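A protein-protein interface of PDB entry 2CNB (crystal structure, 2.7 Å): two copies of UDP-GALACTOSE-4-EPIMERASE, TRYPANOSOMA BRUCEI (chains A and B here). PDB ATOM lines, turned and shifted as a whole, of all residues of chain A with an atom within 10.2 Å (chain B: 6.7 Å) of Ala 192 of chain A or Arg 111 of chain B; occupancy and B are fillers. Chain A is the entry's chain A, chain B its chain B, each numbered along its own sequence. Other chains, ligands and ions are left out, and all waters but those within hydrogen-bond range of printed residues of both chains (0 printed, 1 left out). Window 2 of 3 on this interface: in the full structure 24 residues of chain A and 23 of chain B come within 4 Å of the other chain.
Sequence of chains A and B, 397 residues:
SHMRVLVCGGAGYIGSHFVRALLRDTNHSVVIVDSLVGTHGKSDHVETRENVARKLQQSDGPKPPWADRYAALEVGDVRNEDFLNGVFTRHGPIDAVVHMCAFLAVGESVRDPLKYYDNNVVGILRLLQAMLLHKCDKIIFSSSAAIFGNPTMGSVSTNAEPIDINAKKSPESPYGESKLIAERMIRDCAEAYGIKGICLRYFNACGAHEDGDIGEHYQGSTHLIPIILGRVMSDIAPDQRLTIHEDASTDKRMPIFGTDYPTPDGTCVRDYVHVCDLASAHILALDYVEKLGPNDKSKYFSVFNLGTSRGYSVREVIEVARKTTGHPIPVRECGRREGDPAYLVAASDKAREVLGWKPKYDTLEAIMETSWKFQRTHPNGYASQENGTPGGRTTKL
OH of Tyr 193 of chain A lies within hydrogen-bond range of OD1 of Asp 112 of chain B (2.5 Å).
The backbone nitrogen (N) of Pro 113 of chain B sits close to the side-chain hydroxyl (OH) of Tyr 193 of chain A (3.2 Å).
The guanidinium group of Arg 187 of chain A lies within salt-bridge range of the side-chain carboxylate of Asp 188 of chain A.
Among the printed residues, merely in contact across the chains: Ala 192 of chain A with Pro 113 of chain B (3.4 Å), Ala 192 of chain A with Arg 111 of chain B (3.5 Å), Asp 188 of chain A with Pro 113 of chain B (3.5 Å), Ala 192 of chain A with Val 110 of chain B (3.6 Å) and Asp 188 of chain A with Pro 174 of chain B (3.8 Å).
Of chain B, only Val 110, Arg 111 and Pro 113 come within 4 Å of Ala 192 of chain A.
No residue of chain A comes within 4 Å of Ser 109 of chain B.
Printed residues of chain A within 4 Å of Val 110 of chain B: Ala 192 (3.6 Å).
Printed residues of chain B within 4 Å of Asp 188 of chain A: Pro 113 (3.5 Å) and Pro 174 (3.8 Å).
Of the printed residues of chain A, Pro 174 of chain B touches Asp 188.
Of the printed residues of chain B, Tyr 193 of chain A touches Asp 112 and Pro 113.
The nearest residue of chain B that does not touch Ala 192 of chain A is Asp 112 of chain B (4.4 Å).
The nearest residue of chain A that does not touch Arg 111 of chain B is Tyr 193 of chain A (4.2 Å).
Of the 17 printed residues of chain A, 3 touch a printed residue of chain B.
Hydrophobic or aromatic side chains of chain A that line the printed part of chain B: Ala 192 and Tyr 193.
Printed residues of chain B that touch a printed residue of chain A: Val 110, Arg 111, Asp 112, Pro 113 and Pro 174.
Hydrophobic or aromatic side chains of chain B that line the printed part of chain A: Pro 113 and Pro 174.
Among the printed residues, 7 pairs touch across the chains.
No position is printed for both chains.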
ATOM      1  N   LEU A 132      11.654 -24.903  31.491  1.00  0.00           N
ATOM      2  CA  LEU A 132      11.134 -26.059  30.795  1.00  0.00           C
ATOM      3  C   LEU A 132      11.853 -27.322  31.237  1.00  0.00           C
ATOM      4  O   LEU A 132      11.219 -28.305  31.599  1.00  0.00           O
ATOM      5  CB  LEU A 132      11.261 -25.870  29.287  1.00  0.00           C
ATOM      6  CG  LEU A 132       9.990 -26.224  28.529  1.00  0.00           C
ATOM      7  CD1 LEU A 132       8.743 -26.044  29.397  1.00  0.00           C
ATOM      8  CD2 LEU A 132       9.911 -25.335  27.317  1.00  0.00           C
ATOM      9  N   ARG A 184       6.182 -11.559  24.313  1.00  0.00           N
ATOM     10  CA  ARG A 184       5.740 -12.458  23.250  1.00  0.00           C
ATOM     11  C   ARG A 184       6.224 -13.876  23.497  1.00  0.00           C
ATOM     12  O   ARG A 184       5.437 -14.813  23.460  1.00  0.00           O
ATOM     13  CB  ARG A 184       6.233 -11.981  21.890  1.00  0.00           C
ATOM     14  CG  ARG A 184       5.775 -10.605  21.514  1.00  0.00           C
ATOM     15  CD  ARG A 184       4.273 -10.540  21.371  1.00  0.00           C
ATOM     16  NE  ARG A 184       3.870  -9.309  20.696  1.00  0.00           N
ATOM     17  CZ  ARG A 184       3.016  -8.413  21.187  1.00  0.00           C
ATOM     18  NH1 ARG A 184       2.436  -8.594  22.373  1.00  0.00           N
ATOM     19  NH2 ARG A 184       2.726  -7.332  20.468  1.00  0.00           N
ATOM     20  N   MET A 185       7.516 -14.032  23.756  1.00  0.00           N
ATOM     21  CA  MET A 185       8.055 -15.343  24.053  1.00  0.00           C
ATOM     22  C   MET A 185       7.301 -15.975  25.207  1.00  0.00           C
ATOM     23  O   MET A 185       6.886 -17.108  25.106  1.00  0.00           O
ATOM     24  CB  MET A 185       9.530 -15.245  24.396  1.00  0.00           C
ATOM     25  CG  MET A 185      10.412 -14.892  23.217  1.00  0.00           C
ATOM     26  SD  MET A 185      12.123 -14.698  23.748  1.00  0.00           S
ATOM     27  CE  MET A 185      12.423 -16.297  24.477  1.00  0.00           C
ATOM     28  N   ILE A 186       7.108 -15.227  26.287  1.00  0.00           N
ATOM     29  CA  ILE A 186       6.443 -15.734  27.460  1.00  0.00           C
ATOM     30  C   ILE A 186       5.004 -16.134  27.127  1.00  0.00           C
ATOM     31  O   ILE A 186       4.574 -17.266  27.402  1.00  0.00           O
ATOM     32  CB  ILE A 186       6.517 -14.709  28.583  1.00  0.00           C
ATOM     33  CG1 ILE A 186       7.955 -14.624  29.108  1.00  0.00           C
ATOM     34  CG2 ILE A 186       5.495 -15.011  29.702  1.00  0.00           C
ATOM     35  CD1 ILE A 186       8.269 -13.329  29.905  1.00  0.00           C
ATOM     36  N   ARG A 187       4.278 -15.218  26.493  1.00  0.00           N
ATOM     37  CA  ARG A 187       2.938 -15.503  25.987  1.00  0.00           C
ATOM     38  C   ARG A 187       2.874 -16.801  25.195  1.00  0.00           C
ATOM     39  O   ARG A 187       1.921 -17.545  25.341  1.00  0.00           O
ATOM     40  CB  ARG A 187       2.441 -14.365  25.090  1.00  0.00           C
ATOM     41  CG  ARG A 187       1.026 -14.614  24.540  1.00  0.00           C
ATOM     42  CD  ARG A 187       0.750 -13.862  23.271  1.00  0.00           C
ATOM     43  NE  ARG A 187       1.673 -14.266  22.219  1.00  0.00           N
ATOM     44  CZ  ARG A 187       1.919 -13.551  21.118  1.00  0.00           C
ATOM     45  NH1 ARG A 187       1.317 -12.385  20.933  1.00  0.00           N
ATOM     46  NH2 ARG A 187       2.792 -13.998  20.208  1.00  0.00           N
ATOM     47  N   ASP A 188       3.870 -17.046  24.340  1.00  0.00           N
ATOM     48  CA  ASP A 188       3.835 -18.180  23.411  1.00  0.00           C
ATOM     49  C   ASP A 188       4.138 -19.480  24.114  1.00  0.00           C
ATOM     50  O   ASP A 188       3.743 -20.551  23.664  1.00  0.00           O
ATOM     51  CB  ASP A 188       4.739 -17.953  22.199  1.00  0.00           C
ATOM     52  CG  ASP A 188       4.161 -16.919  21.232  1.00  0.00           C
ATOM     53  OD1 ASP A 188       2.942 -16.619  21.339  1.00  0.00           O
ATOM     54  OD2 ASP A 188       4.915 -16.381  20.383  1.00  0.00           O
ATOM     55  N   CYS A 189       4.803 -19.366  25.252  1.00  0.00           N
ATOM     56  CA  CYS A 189       5.095 -20.511  26.090  1.00  0.00           C
ATOM     57  C   CYS A 189       3.848 -20.932  26.855  1.00  0.00           C
ATOM     58  O   CYS A 189       3.743 -22.083  27.289  1.00  0.00           O
ATOM     59  CB  CYS A 189       6.256 -20.183  27.041  1.00  0.00           C
ATOM     60  SG  CYS A 189       7.815 -19.957  26.169  1.00  0.00           S
ATOM     61  N   ALA A 190       2.901 -20.013  27.018  1.00  0.00           N
ATOM     62  CA  ALA A 190       1.668 -20.360  27.709  1.00  0.00           C
ATOM     63  C   ALA A 190       0.915 -21.479  26.970  1.00  0.00           C
ATOM     64  O   ALA A 190       0.713 -22.567  27.534  1.00  0.00           O
ATOM     65  CB  ALA A 190       0.787 -19.138  27.903  1.00  0.00           C
ATOM     66  N   GLU A 191       0.542 -21.228  25.707  1.00  0.00           N
ATOM     67  CA  GLU A 191      -0.234 -22.197  24.918  1.00  0.00           C
ATOM     68  C   GLU A 191       0.567 -23.483  24.679  1.00  0.00           C
ATOM     69  O   GLU A 191      -0.005 -24.578  24.639  1.00  0.00           O
ATOM     70  CB  GLU A 191      -0.709 -21.551  23.589  1.00  0.00           C
ATOM     71  CG  GLU A 191      -1.444 -22.454  22.567  1.00  0.00           C
ATOM     72  CD  GLU A 191      -2.661 -23.218  23.131  1.00  0.00           C
ATOM     73  OE1 GLU A 191      -3.499 -22.630  23.860  1.00  0.00           O
ATOM     74  OE2 GLU A 191      -2.783 -24.427  22.819  1.00  0.00           O
ATOM     75  N   ALA A 192       1.885 -23.342  24.534  1.00  0.00           N
ATOM     76  CA  ALA A 192       2.715 -24.442  24.125  1.00  0.00           C
ATOM     77  C   ALA A 192       3.086 -25.381  25.253  1.00  0.00           C
ATOM     78  O   ALA A 192       3.105 -26.586  25.064  1.00  0.00           O
ATOM     79  CB  ALA A 192       3.941 -23.931  23.431  1.00  0.00           C
ATOM     80  N   TYR A 193       3.395 -24.836  26.423  1.00  0.00           N
ATOM     81  CA  TYR A 193       3.986 -25.648  27.491  1.00  0.00           C
ATOM     82  C   TYR A 193       3.233 -25.531  28.816  1.00  0.00           C
ATOM     83  O   TYR A 193       3.642 -26.142  29.804  1.00  0.00           O
ATOM     84  CB  TYR A 193       5.454 -25.256  27.740  1.00  0.00           C
ATOM     85  CG  TYR A 193       6.323 -25.046  26.526  1.00  0.00           C
ATOM     86  CD1 TYR A 193       6.772 -26.124  25.754  1.00  0.00           C
ATOM     87  CD2 TYR A 193       6.721 -23.760  26.161  1.00  0.00           C
ATOM     88  CE1 TYR A 193       7.584 -25.922  24.642  1.00  0.00           C
ATOM     89  CE2 TYR A 193       7.529 -23.542  25.053  1.00  0.00           C
ATOM     90  CZ  TYR A 193       7.964 -24.616  24.288  1.00  0.00           C
ATOM     91  OH  TYR A 193       8.787 -24.368  23.186  1.00  0.00           O
ATOM     92  N   GLY A 194       2.168 -24.726  28.846  1.00  0.00           N
ATOM     93  CA  GLY A 194       1.435 -24.472  30.087  1.00  0.00           C
ATOM     94  C   GLY A 194       2.168 -23.576  31.090  1.00  0.00           C
ATOM     95  O   GLY A 194       1.816 -23.529  32.267  1.00  0.00           O
ATOM     96  N   ILE A 195       3.184 -22.843  30.647  1.00  0.00           N
ATOM     97  CA  ILE A 195       3.844 -21.884  31.528  1.00  0.00           C
ATOM     98  C   ILE A 195       2.898 -20.741  31.894  1.00  0.00           C
ATOM     99  O   ILE A 195       2.157 -20.269  31.047  1.00  0.00           O
ATOM    100  CB  ILE A 195       5.161 -21.372  30.904  1.00  0.00           C
ATOM    101  CG1 ILE A 195       6.215 -22.498  30.998  1.00  0.00           C
ATOM    102  CG2 ILE A 195       5.613 -20.052  31.581  1.00  0.00           C
ATOM    103  CD1 ILE A 195       7.586 -22.114  30.545  1.00  0.00           C
ATOM    104  N   LYS A 196       2.920 -20.332  33.167  1.00  0.00           N
ATOM    105  CA  LYS A 196       2.009 -19.322  33.730  1.00  0.00           C
ATOM    106  C   LYS A 196       2.785 -18.049  33.977  1.00  0.00           C
ATOM    107  O   LYS A 196       3.601 -17.979  34.898  1.00  0.00           O
ATOM    108  CB  LYS A 196       1.400 -19.826  35.040  1.00  0.00           C
ATOM    109  CG  LYS A 196       0.621 -21.088  34.879  1.00  0.00           C
ATOM    110  CD  LYS A 196       0.250 -21.658  36.196  1.00  0.00           C
ATOM    111  CE  LYS A 196      -0.350 -23.040  35.995  1.00  0.00           C
ATOM    112  NZ  LYS A 196      -0.285 -23.869  37.226  1.00  0.00           N
ATOM    113  N   LYS A 297      -7.604 -21.908  30.931  1.00  0.00           N
ATOM    114  CA  LYS A 297      -6.203 -21.699  31.248  1.00  0.00           C
ATOM    115  C   LYS A 297      -5.882 -20.525  30.307  1.00  0.00           C
ATOM    116  O   LYS A 297      -4.739 -20.234  29.957  1.00  0.00           O
ATOM    117  CB  LYS A 297      -5.382 -22.952  30.922  1.00  0.00           C
ATOM    118  CG  LYS A 297      -5.523 -23.474  29.490  1.00  0.00           C
ATOM    119  CD  LYS A 297      -4.816 -24.802  29.321  1.00  0.00           C
ATOM    120  CE  LYS A 297      -3.359 -24.590  28.898  1.00  0.00           C
ATOM    121  NZ  LYS A 297      -2.482 -25.801  29.115  1.00  0.00           N
ATOM    122  N   TYR A 300      -3.512 -18.140  31.889  1.00  0.00           N
ATOM    123  CA  TYR A 300      -2.111 -18.512  32.062  1.00  0.00           C
ATOM    124  C   TYR A 300      -1.129 -17.386  31.711  1.00  0.00           C
ATOM    125  O   TYR A 300      -0.017 -17.344  32.240  1.00  0.00           O
ATOM    126  CB  TYR A 300      -1.797 -19.816  31.301  1.00  0.00           C
ATOM    127  CG  TYR A 300      -2.050 -21.110  32.092  1.00  0.00           C
ATOM    128  CD1 TYR A 300      -3.131 -21.224  32.980  1.00  0.00           C
ATOM    129  CD2 TYR A 300      -1.215 -22.221  31.931  1.00  0.00           C
ATOM    130  CE1 TYR A 300      -3.359 -22.392  33.692  1.00  0.00           C
ATOM    131  CE2 TYR A 300      -1.437 -23.397  32.628  1.00  0.00           C
ATOM    132  CZ  TYR A 300      -2.512 -23.484  33.517  1.00  0.00           C
ATOM    133  OH  TYR A 300      -2.732 -24.667  34.237  1.00  0.00           O
ATOM    134  N   PHE A 301      -1.544 -16.471  30.837  1.00  0.00           N
ATOM    135  CA  PHE A 301      -0.749 -15.287  30.522  1.00  0.00           C
ATOM    136  C   PHE A 301      -1.576 -14.050  30.773  1.00  0.00           C
ATOM    137  O   PHE A 301      -2.678 -13.919  30.254  1.00  0.00           O
ATOM    138  CB  PHE A 301      -0.282 -15.314  29.075  1.00  0.00           C
ATOM    139  CG  PHE A 301       0.537 -14.127  28.680  1.00  0.00           C
ATOM    140  CD1 PHE A 301       1.891 -14.064  28.998  1.00  0.00           C
ATOM    141  CD2 PHE A 301      -0.048 -13.055  27.983  1.00  0.00           C
ATOM    142  CE1 PHE A 301       2.642 -12.951  28.628  1.00  0.00           C
ATOM    143  CE2 PHE A 301       0.702 -11.935  27.614  1.00  0.00           C
ATOM    144  CZ  PHE A 301       2.038 -11.878  27.932  1.00  0.00           C
ATOM    145  N   VAL B 106       5.543 -23.443  10.244  1.00  0.00           N
ATOM    146  CA  VAL B 106       4.597 -22.565  10.947  1.00  0.00           C
ATOM    147  C   VAL B 106       3.883 -23.297  12.087  1.00  0.00           C
ATOM    148  O   VAL B 106       3.756 -22.768  13.183  1.00  0.00           O
ATOM    149  CB  VAL B 106       3.590 -21.836   9.985  1.00  0.00           C
ATOM    150  CG1 VAL B 106       2.373 -21.335  10.747  1.00  0.00           C
ATOM    151  CG2 VAL B 106       4.259 -20.658   9.319  1.00  0.00           C
ATOM    152  N   GLY B 107       3.442 -24.521  11.800  1.00  0.00           N
ATOM    153  CA  GLY B 107       2.786 -25.405  12.766  1.00  0.00           C
ATOM    154  C   GLY B 107       3.673 -25.736  13.945  1.00  0.00           C
ATOM    155  O   GLY B 107       3.293 -25.492  15.096  1.00  0.00           O
ATOM    156  N   GLU B 108       4.857 -26.278  13.670  1.00  0.00           N
ATOM    157  CA  GLU B 108       5.795 -26.612  14.743  1.00  0.00           C
ATOM    158  C   GLU B 108       6.094 -25.396  15.641  1.00  0.00           C
ATOM    159  O   GLU B 108       6.143 -25.516  16.867  1.00  0.00           O
ATOM    160  CB  GLU B 108       7.079 -27.213  14.177  1.00  0.00           C
ATOM    161  CG  GLU B 108       8.007 -27.768  15.233  1.00  0.00           C
ATOM    162  CD  GLU B 108       9.451 -27.898  14.750  1.00  0.00           C
ATOM    163  OE1 GLU B 108       9.857 -27.184  13.805  1.00  0.00           O
ATOM    164  OE2 GLU B 108      10.195 -28.707  15.335  1.00  0.00           O
ATOM    165  N   SER B 109       6.251 -24.226  15.033  1.00  0.00           N
ATOM    166  CA  SER B 109       6.473 -22.999  15.799  1.00  0.00           C
ATOM    167  C   SER B 109       5.415 -22.742  16.901  1.00  0.00           C
ATOM    168  O   SER B 109       5.754 -22.282  17.989  1.00  0.00           O
ATOM    169  CB  SER B 109       6.660 -21.776  14.877  1.00  0.00           C
ATOM    170  OG  SER B 109       5.429 -21.263  14.384  1.00  0.00           O
ATOM    171  N   VAL B 110       4.148 -23.051  16.637  1.00  0.00           N
ATOM    172  CA  VAL B 110       3.086 -22.845  17.635  1.00  0.00           C
ATOM    173  C   VAL B 110       3.238 -23.832  18.793  1.00  0.00           C
ATOM    174  O   VAL B 110       3.029 -23.486  19.951  1.00  0.00           O
ATOM    175  CB  VAL B 110       1.656 -22.937  16.998  1.00  0.00           C
ATOM    176  CG1 VAL B 110       0.558 -22.724  18.043  1.00  0.00           C
ATOM    177  CG2 VAL B 110       1.503 -21.911  15.865  1.00  0.00           C
ATOM    178  N   ARG B 111       3.634 -25.055  18.462  1.00  0.00           N
ATOM    179  CA  ARG B 111       3.731 -26.136  19.424  1.00  0.00           C
ATOM    180  C   ARG B 111       4.972 -26.016  20.293  1.00  0.00           C
ATOM    181  O   ARG B 111       5.000 -26.528  21.421  1.00  0.00           O
ATOM    182  CB  ARG B 111       3.754 -27.476  18.687  1.00  0.00           C
ATOM    183  CG  ARG B 111       2.441 -28.241  18.731  1.00  0.00           C
ATOM    184  CD  ARG B 111       2.600 -29.625  18.094  1.00  0.00           C
ATOM    185  NE  ARG B 111       2.310 -29.569  16.662  1.00  0.00           N
ATOM    186  CZ  ARG B 111       3.223 -29.625  15.694  1.00  0.00           C
ATOM    187  NH1 ARG B 111       4.512 -29.772  16.004  1.00  0.00           N
ATOM    188  NH2 ARG B 111       2.837 -29.544  14.412  1.00  0.00           N
ATOM    189  N   ASP B 112       5.994 -25.339  19.768  1.00  0.00           N
ATOM    190  CA  ASP B 112       7.315 -25.344  20.392  1.00  0.00           C
ATOM    191  C   ASP B 112       8.112 -24.048  20.065  1.00  0.00           C
ATOM    192  O   ASP B 112       9.120 -24.077  19.335  1.00  0.00           O
ATOM    193  CB  ASP B 112       8.047 -26.616  19.951  1.00  0.00           C
ATOM    194  CG  ASP B 112       9.394 -26.793  20.614  1.00  0.00           C
ATOM    195  OD1 ASP B 112       9.663 -26.248  21.712  1.00  0.00           O
ATOM    196  OD2 ASP B 112      10.208 -27.499  20.012  1.00  0.00           O
ATOM    197  N   PRO B 113       7.653 -22.908  20.605  1.00  0.00           N
ATOM    198  CA  PRO B 113       8.193 -21.617  20.215  1.00  0.00           C
ATOM    199  C   PRO B 113       9.674 -21.427  20.498  1.00  0.00           C
ATOM    200  O   PRO B 113      10.377 -20.835  19.662  1.00  0.00           O
ATOM    201  CB  PRO B 113       7.371 -20.622  21.041  1.00  0.00           C
ATOM    202  CG  PRO B 113       6.790 -21.385  22.117  1.00  0.00           C
ATOM    203  CD  PRO B 113       6.564 -22.752  21.583  1.00  0.00           C
ATOM    204  N   PRO B 174       4.660 -18.002  16.242  1.00  0.00           N
ATOM    205  CA  PRO B 174       6.015 -17.735  16.712  1.00  0.00           C
ATOM    206  C   PRO B 174       7.037 -17.599  15.571  1.00  0.00           C
ATOM    207  O   PRO B 174       7.968 -16.785  15.681  1.00  0.00           O
ATOM    208  CB  PRO B 174       6.330 -18.955  17.594  1.00  0.00           C
ATOM    209  CG  PRO B 174       5.013 -19.430  18.055  1.00  0.00           C
ATOM    210  CD  PRO B 174       4.074 -19.182  16.904  1.00  0.00           C
ATOM    211  N   ARG B 337      -4.676 -26.107  10.912  1.00  0.00           N
ATOM    212  CA  ARG B 337      -3.334 -26.107  11.462  1.00  0.00           C
ATOM    213  C   ARG B 337      -3.125 -24.751  12.105  1.00  0.00           C
ATOM    214  O   ARG B 337      -3.193 -23.720  11.426  1.00  0.00           O
ATOM    215  CB  ARG B 337      -2.315 -26.289  10.338  1.00  0.00           C
ATOM    216  CG  ARG B 337      -0.921 -26.501  10.815  1.00  0.00           C
ATOM    217  CD  ARG B 337      -0.028 -25.660   9.994  1.00  0.00           C
ATOM    218  NE  ARG B 337       0.586 -26.386   8.896  1.00  0.00           N
ATOM    219  CZ  ARG B 337       1.122 -25.796   7.834  1.00  0.00           C
ATOM    220  NH1 ARG B 337       1.088 -24.469   7.718  1.00  0.00           N
ATOM    221  NH2 ARG B 337       1.668 -26.543   6.868  1.00  0.00           N
